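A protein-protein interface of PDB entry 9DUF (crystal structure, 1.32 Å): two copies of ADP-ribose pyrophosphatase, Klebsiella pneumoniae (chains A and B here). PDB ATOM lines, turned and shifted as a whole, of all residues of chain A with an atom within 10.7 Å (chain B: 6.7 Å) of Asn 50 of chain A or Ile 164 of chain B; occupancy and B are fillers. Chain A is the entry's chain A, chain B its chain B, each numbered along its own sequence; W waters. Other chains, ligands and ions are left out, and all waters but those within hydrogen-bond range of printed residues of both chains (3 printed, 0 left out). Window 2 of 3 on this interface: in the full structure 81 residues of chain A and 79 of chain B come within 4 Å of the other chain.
The backbone NH (N) of His 165 of chain B lies within hydrogen-bond range of the backbone carbonyl oxygen (O) of Ile 174 of chain B.
OG1 of Thr 18 of chain A is in hydrogen-bond range of NH1 of Arg 175 of chain B, 2.9 Å away.
N of Phe 49 of chain A is in hydrogen-bond range of OD2 of Asp 173 of chain B (2.9 Å).
No position is printed for both chains.
Of the 7 pairs that touch across the chains among the printed residues, none has its exchanged pair printed and touching as well.
Water W1 lies within hydrogen-bond range of O of Gly 16 of chain A (2.5 Å), OG1 of Thr 18 of chain A (3.0 Å) and NH1 of Arg 175 of chain B (3.3 Å).
Water W3 lies within hydrogen-bond range of OD1 of Asp 173 of chain B (2.7 Å), N of Asn 50 of chain A (2.9 Å) and N of Phe 49 of chain A (3.3 Å).
Water W2 bridges OD2 of Asp 173 of chain B and O of Arg 47 of chain A.
Printed residues of chain A that touch a printed residue of chain B: Thr 18, Leu 48, Phe 49 and Asn 50.
Along chain A the printed residues that touch a printed residue of chain B span positions 18 to 50.
Hydrophobic or aromatic side chains of chain B that line the printed part of chain A: Ile 164.
Among the printed residues, 7 pairs touch across the chains.
Of the printed residues of chain B, Thr 18 of chain A touches Arg 175 (2.9 Å).
Asn 50 of chain A touches just one residue of chain B: Ile 164.
No residue of chain A comes within 4 Å of Gly 163 of chain B.
Of the printed residues of chain A, Ile 164 of chain B touches Phe 49 (3.6 Å) and Asn 50 (3.6 Å).
No residue of chain A comes within 4 Å of His 165 of chain B.
No residue of chain A comes within 4 Å of Gly 166 of chain B.
Of the printed residues of chain A, Asp 173 of chain B touches Leu 48 (3.2 Å) and Phe 49 (2.9 Å).
Printed residues of chain A within 4 Å of Ile 174 of chain B: Phe 49.
The nearest residue of chain B that does not touch Asn 50 of chain A is Asp 173 of chain B (5.0 Å).
The nearest printed residue of chain A that does not touch Asp 173 of chain B is Arg 47 of chain A (4.2 Å).
Among the printed residues, pairs that only touch across the chains: Leu 48 of chain A with Asp 173 of chain B (3.2 Å), Phe 49 of chain A with Ile 164 of chain B (3.6 Å), Phe 49 of chain A with Ile 174 of chain B (3.7 Å), Phe 49 of chain A with Arg 175 of chain B (3.4 Å) and Asn 50 of chain A with Ile 164 of chain B (3.6 Å).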
ATOM      1  N   GLY A  16      -0.463   3.635  27.816  1.00  0.00           N
ATOM      2  CA  GLY A  16      -0.132   2.511  28.657  1.00  0.00           C
ATOM      3  C   GLY A  16       1.071   1.756  28.125  1.00  0.00           C
ATOM      4  O   GLY A  16       1.777   2.201  27.217  1.00  0.00           O
ATOM      5  N   THR A  18       3.524  -1.075  26.386  1.00  0.00           N
ATOM      6  CA  THR A  18       3.745  -1.334  24.976  1.00  0.00           C
ATOM      7  C   THR A  18       3.691  -2.816  24.645  1.00  0.00           C
ATOM      8  O   THR A  18       3.185  -3.191  23.578  1.00  0.00           O
ATOM      9  CB  THR A  18       5.123  -0.775  24.589  1.00  0.00           C
ATOM     10  OG1 THR A  18       5.201   0.617  24.923  1.00  0.00           O
ATOM     11  CG2 THR A  18       5.379  -0.926  23.101  1.00  0.00           C
ATOM     12  N   PHE A  19       4.172  -3.669  25.551  1.00  0.00           N
ATOM     13  CA  PHE A  19       4.354  -5.087  25.281  1.00  0.00           C
ATOM     14  C   PHE A  19       3.687  -5.937  26.354  1.00  0.00           C
ATOM     15  O   PHE A  19       3.435  -5.479  27.478  1.00  0.00           O
ATOM     16  CB  PHE A  19       5.848  -5.435  25.196  1.00  0.00           C
ATOM     17  CG  PHE A  19       6.562  -4.776  24.043  1.00  0.00           C
ATOM     18  CD1 PHE A  19       6.137  -4.977  22.741  1.00  0.00           C
ATOM     19  CD2 PHE A  19       7.662  -3.961  24.266  1.00  0.00           C
ATOM     20  CE1 PHE A  19       6.792  -4.373  21.683  1.00  0.00           C
ATOM     21  CE2 PHE A  19       8.323  -3.359  23.208  1.00  0.00           C
ATOM     22  CZ  PHE A  19       7.887  -3.572  21.914  1.00  0.00           C
ATOM     23  N   HIS A  46      13.558 -10.628  25.067  1.00  0.00           N
ATOM     24  CA  HIS A  46      12.339  -9.836  24.992  1.00  0.00           C
ATOM     25  C   HIS A  46      12.379  -8.835  23.846  1.00  0.00           C
ATOM     26  O   HIS A  46      13.441  -8.431  23.377  1.00  0.00           O
ATOM     27  CB  HIS A  46      12.092  -9.089  26.315  1.00  0.00           C
ATOM     28  CG  HIS A  46      13.152  -8.083  26.659  1.00  0.00           C
ATOM     29  ND1 HIS A  46      13.117  -6.784  26.202  1.00  0.00           N
ATOM     30  CD2 HIS A  46      14.269  -8.185  27.419  1.00  0.00           C
ATOM     31  CE1 HIS A  46      14.172  -6.131  26.660  1.00  0.00           C
ATOM     32  NE2 HIS A  46      14.883  -6.956  27.406  1.00  0.00           N
ATOM     33  N   ARG A  47      11.189  -8.415  23.418  1.00  0.00           N
ATOM     34  CA  ARG A  47      11.084  -7.407  22.376  1.00  0.00           C
ATOM     35  C   ARG A  47      11.685  -6.084  22.836  1.00  0.00           C
ATOM     36  O   ARG A  47      11.566  -5.688  24.002  1.00  0.00           O
ATOM     37  CB  ARG A  47       9.616  -7.185  22.012  1.00  0.00           C
ATOM     38  CG  ARG A  47       8.991  -8.324  21.223  1.00  0.00           C
ATOM     39  CD  ARG A  47       9.256  -8.208  19.726  1.00  0.00           C
ATOM     40  NE  ARG A  47       8.315  -7.295  19.084  1.00  0.00           N
ATOM     41  CZ  ARG A  47       8.589  -6.049  18.712  1.00  0.00           C
ATOM     42  NH1 ARG A  47       9.790  -5.518  18.885  1.00  0.00           N
ATOM     43  NH2 ARG A  47       7.632  -5.320  18.143  1.00  0.00           N
ATOM     44  N   LEU A  48      12.279  -5.377  21.877  1.00  0.00           N
ATOM     45  CA  LEU A  48      12.855  -4.059  22.077  1.00  0.00           C
ATOM     46  C   LEU A  48      11.928  -3.007  21.489  1.00  0.00           C
ATOM     47  O   LEU A  48      11.243  -3.248  20.489  1.00  0.00           O
ATOM     48  CB  LEU A  48      14.224  -3.980  21.397  1.00  0.00           C
ATOM     49  CG  LEU A  48      15.204  -5.056  21.874  1.00  0.00           C
ATOM     50  CD1 LEU A  48      16.404  -5.159  20.941  1.00  0.00           C
ATOM     51  CD2 LEU A  48      15.670  -4.784  23.305  1.00  0.00           C
ATOM     52  N   PHE A  49      11.930  -1.823  22.113  1.00  0.00           N
ATOM     53  CA  PHE A  49      11.039  -0.751  21.670  1.00  0.00           C
ATOM     54  C   PHE A  49      11.297  -0.334  20.228  1.00  0.00           C
ATOM     55  O   PHE A  49      10.348  -0.023  19.499  1.00  0.00           O
ATOM     56  CB  PHE A  49      11.165   0.455  22.598  1.00  0.00           C
ATOM     57  CG  PHE A  49      10.580   0.216  23.958  1.00  0.00           C
ATOM     58  CD1 PHE A  49       9.213   0.037  24.123  1.00  0.00           C
ATOM     59  CD2 PHE A  49      11.392   0.184  25.077  1.00  0.00           C
ATOM     60  CE1 PHE A  49       8.675  -0.179  25.381  1.00  0.00           C
ATOM     61  CE2 PHE A  49      10.859  -0.039  26.336  1.00  0.00           C
ATOM     62  CZ  PHE A  49       9.508  -0.219  26.490  1.00  0.00           C
ATOM     63  N   ASN A  50      12.564  -0.269  19.809  1.00  0.00           N
ATOM     64  CA  ASN A  50      12.894   0.148  18.451  1.00  0.00           C
ATOM     65  C   ASN A  50      12.805  -1.006  17.467  1.00  0.00           C
ATOM     66  O   ASN A  50      13.161  -0.841  16.295  1.00  0.00           O
ATOM     67  CB  ASN A  50      14.298   0.776  18.392  1.00  0.00           C
ATOM     68  CG  ASN A  50      14.360   2.190  19.000  1.00  0.00           C
ATOM     69  OD1 ASN A  50      15.293   2.518  19.740  1.00  0.00           O
ATOM     70  ND2 ASN A  50      13.370   3.020  18.691  1.00  0.00           N
ATOM     71  N   GLY A  51      12.339  -2.160  17.909  1.00  0.00           N
ATOM     72  CA  GLY A  51      12.153  -3.289  17.024  1.00  0.00           C
ATOM     73  C   GLY A  51      13.172  -4.384  17.283  1.00  0.00           C
ATOM     74  O   GLY A  51      14.304  -4.135  17.725  1.00  0.00           O
ATOM     75  N   GLY A  52      12.763  -5.615  17.013  1.00  0.00           N
ATOM     76  CA  GLY A  52      13.640  -6.750  17.180  1.00  0.00           C
ATOM     77  C   GLY A  52      13.594  -7.303  18.588  1.00  0.00           C
ATOM     78  O   GLY A  52      12.825  -6.869  19.448  1.00  0.00           O
ATOM     79  N   MET A  53      14.462  -8.280  18.820  1.00  0.00           N
ATOM     80  CA  MET A  53      14.539  -9.013  20.073  1.00  0.00           C
ATOM     81  C   MET A  53      15.900  -8.805  20.721  1.00  0.00           C
ATOM     82  O   MET A  53      16.930  -8.773  20.041  1.00  0.00           O
ATOM     83  CB  MET A  53      14.373 -10.521  19.833  1.00  0.00           C
ATOM     84  CG  MET A  53      12.979 -10.955  19.441  1.00  0.00           C
ATOM     85  SD  MET A  53      11.763 -10.704  20.741  1.00  0.00           S
ATOM     86  CE  MET A  53      12.286 -11.900  21.954  1.00  0.00           C
ATOM     87  N   SER A  54      15.902  -8.703  22.043  1.00  0.00           N
ATOM     88  CA  SER A  54      17.142  -8.702  22.791  1.00  0.00           C
ATOM     89  C   SER A  54      17.837 -10.050  22.623  1.00  0.00           C
ATOM     90  O   SER A  54      17.260 -11.027  22.151  1.00  0.00           O
ATOM     91  CB  SER A  54      16.859  -8.509  24.277  1.00  0.00           C
ATOM     92  OG  SER A  54      16.386  -9.714  24.866  1.00  0.00           O
ATOM     93  N   GLU B 123      20.279   9.094  31.609  1.00  0.00           N
ATOM     94  CA  GLU B 123      20.451   7.833  30.892  1.00  0.00           C
ATOM     95  C   GLU B 123      19.122   7.198  30.525  1.00  0.00           C
ATOM     96  O   GLU B 123      19.001   6.563  29.472  1.00  0.00           O
ATOM     97  CB  GLU B 123      21.245   6.839  31.733  1.00  0.00           C
ATOM     98  CG  GLU B 123      22.667   7.252  32.003  1.00  0.00           C
ATOM     99  CD  GLU B 123      23.433   6.257  32.857  1.00  0.00           C
ATOM    100  OE1 GLU B 123      22.817   5.303  33.385  1.00  0.00           O
ATOM    101  OE2 GLU B 123      24.654   6.437  32.994  1.00  0.00           O
ATOM    102  N   GLU B 124      18.132   7.322  31.400  1.00  0.00           N
ATOM    103  CA  GLU B 124      16.876   6.603  31.248  1.00  0.00           C
ATOM    104  C   GLU B 124      15.780   7.432  30.613  1.00  0.00           C
ATOM    105  O   GLU B 124      14.821   6.860  30.090  1.00  0.00           O
ATOM    106  CB  GLU B 124      16.399   6.129  32.619  1.00  0.00           C
ATOM    107  CG  GLU B 124      17.390   5.228  33.278  1.00  0.00           C
ATOM    108  CD  GLU B 124      16.829   4.440  34.444  1.00  0.00           C
ATOM    109  OE1 GLU B 124      15.774   4.849  34.994  1.00  0.00           O
ATOM    110  OE2 GLU B 124      17.466   3.416  34.830  1.00  0.00           O
ATOM    111  N   LYS B 162      11.059  12.366  26.079  1.00  0.00           N
ATOM    112  CA  LYS B 162      10.429  11.614  24.997  1.00  0.00           C
ATOM    113  C   LYS B 162      11.420  10.614  24.448  1.00  0.00           C
ATOM    114  O   LYS B 162      12.625  10.826  24.526  1.00  0.00           O
ATOM    115  CB  LYS B 162       9.966  12.542  23.864  1.00  0.00           C
ATOM    116  CG  LYS B 162      11.076  13.399  23.312  1.00  0.00           C
ATOM    117  CD  LYS B 162      10.535  14.584  22.533  1.00  0.00           C
ATOM    118  CE  LYS B 162      10.985  15.876  23.165  1.00  0.00           C
ATOM    119  NZ  LYS B 162      10.408  17.081  22.534  1.00  0.00           N
ATOM    120  N   GLY B 163      10.905   9.528  23.900  1.00  0.00           N
ATOM    121  CA  GLY B 163      11.718   8.611  23.130  1.00  0.00           C
ATOM    122  C   GLY B 163      12.191   7.407  23.915  1.00  0.00           C
ATOM    123  O   GLY B 163      11.704   7.078  25.002  1.00  0.00           O
ATOM    124  N   ILE B 164      13.150   6.716  23.306  1.00  0.00           N
ATOM    125  CA  ILE B 164      13.695   5.454  23.796  1.00  0.00           C
ATOM    126  C   ILE B 164      15.100   5.713  24.319  1.00  0.00           C
ATOM    127  O   ILE B 164      15.937   6.297  23.607  1.00  0.00           O
ATOM    128  CB  ILE B 164      13.730   4.405  22.670  1.00  0.00           C
ATOM    129  CG1 ILE B 164      12.339   4.202  22.062  1.00  0.00           C
ATOM    130  CG2 ILE B 164      14.280   3.095  23.179  1.00  0.00           C
ATOM    131  CD1 ILE B 164      11.242   3.986  23.072  1.00  0.00           C
ATOM    132  N   HIS B 165      15.351   5.262  25.543  1.00  0.00           N
ATOM    133  CA  HIS B 165      16.573   5.544  26.270  1.00  0.00           C
ATOM    134  C   HIS B 165      17.019   4.241  26.926  1.00  0.00           C
ATOM    135  O   HIS B 165      16.625   3.140  26.520  1.00  0.00           O
ATOM    136  CB  HIS B 165      16.328   6.682  27.272  1.00  0.00           C
ATOM    137  CG  HIS B 165      15.933   7.967  26.617  1.00  0.00           C
ATOM    138  ND1 HIS B 165      16.853   8.927  26.257  1.00  0.00           N
ATOM    139  CD2 HIS B 165      14.727   8.440  26.233  1.00  0.00           C
ATOM    140  CE1 HIS B 165      16.231   9.941  25.686  1.00  0.00           C
ATOM    141  NE2 HIS B 165      14.941   9.665  25.648  1.00  0.00           N
ATOM    142  N   GLY B 166      17.821   4.366  27.970  1.00  0.00           N
ATOM    143  CA  GLY B 166      18.490   3.226  28.555  1.00  0.00           C
ATOM    144  C   GLY B 166      19.827   2.968  27.894  1.00  0.00           C
ATOM    145  O   GLY B 166      20.060   3.315  26.741  1.00  0.00           O
ATOM    146  N   ASP B 173      16.452  -1.173  28.156  1.00  0.00           N
ATOM    147  CA  ASP B 173      15.649  -0.675  27.036  1.00  0.00           C
ATOM    148  C   ASP B 173      14.421  -0.006  27.643  1.00  0.00           C
ATOM    149  O   ASP B 173      13.592  -0.679  28.263  1.00  0.00           O
ATOM    150  CB  ASP B 173      15.266  -1.836  26.116  1.00  0.00           C
ATOM    151  CG  ASP B 173      14.529  -1.394  24.859  1.00  0.00           C
ATOM    152  OD1 ASP B 173      14.991  -0.456  24.174  1.00  0.00           O
ATOM    153  OD2 ASP B 173      13.501  -2.029  24.530  1.00  0.00           O
ATOM    154  N   ILE B 174      14.316   1.315  27.483  1.00  0.00           N
ATOM    155  CA  ILE B 174      13.404   2.141  28.270  1.00  0.00           C
ATOM    156  C   ILE B 174      12.634   3.070  27.348  1.00  0.00           C
ATOM    157  O   ILE B 174      13.235   3.760  26.521  1.00  0.00           O
ATOM    158  CB  ILE B 174      14.167   2.965  29.321  1.00  0.00           C
ATOM    159  CG1 ILE B 174      14.892   2.006  30.265  1.00  0.00           C
ATOM    160  CG2 ILE B 174      13.215   3.852  30.107  1.00  0.00           C
ATOM    161  CD1 ILE B 174      15.763   2.672  31.299  1.00  0.00           C
ATOM    162  N   ARG B 175      11.320   3.129  27.521  1.00  0.00           N
ATOM    163  CA  ARG B 175      10.469   4.054  26.784  1.00  0.00           C
ATOM    164  C   ARG B 175       9.921   5.118  27.727  1.00  0.00           C
ATOM    165  O   ARG B 175       9.356   4.798  28.776  1.00  0.00           O
ATOM    166  CB  ARG B 175       9.316   3.320  26.100  1.00  0.00           C
ATOM    167  CG  ARG B 175       8.378   4.240  25.322  1.00  0.00           C
ATOM    168  CD  ARG B 175       7.311   3.458  24.568  1.00  0.00           C
ATOM    169  NE  ARG B 175       6.448   4.348  23.804  1.00  0.00           N
ATOM    170  CZ  ARG B 175       5.494   3.941  22.983  1.00  0.00           C
ATOM    171  NH1 ARG B 175       5.240   2.655  22.807  1.00  0.00           N
ATOM    172  NH2 ARG B 175       4.796   4.847  22.299  1.00  0.00           N
ATOM    173  N   VAL B 176      10.051   6.371  27.338  1.00  0.00           N
ATOM    174  CA  VAL B 176       9.522   7.476  28.130  1.00  0.00           C
ATOM    175  C   VAL B 176       8.046   7.674  27.835  1.00  0.00           C
ATOM    176  O   VAL B 176       7.619   7.666  26.677  1.00  0.00           O
ATOM    177  CB  VAL B 176      10.312   8.765  27.850  1.00  0.00           C
ATOM    178  CG1 VAL B 176       9.608   9.986  28.455  1.00  0.00           C
ATOM    179  CG2 VAL B 176      11.741   8.630  28.363  1.00  0.00           C
HETATM  180  O   HOH W   1       2.669   2.141  24.891  1.00  0.00           O
HETATM  181  O   HOH W   2      11.639  -3.587  25.824  1.00  0.00           O
HETATM  182  O   HOH W   3      14.874  -0.402  21.524  1.00  0.00           O
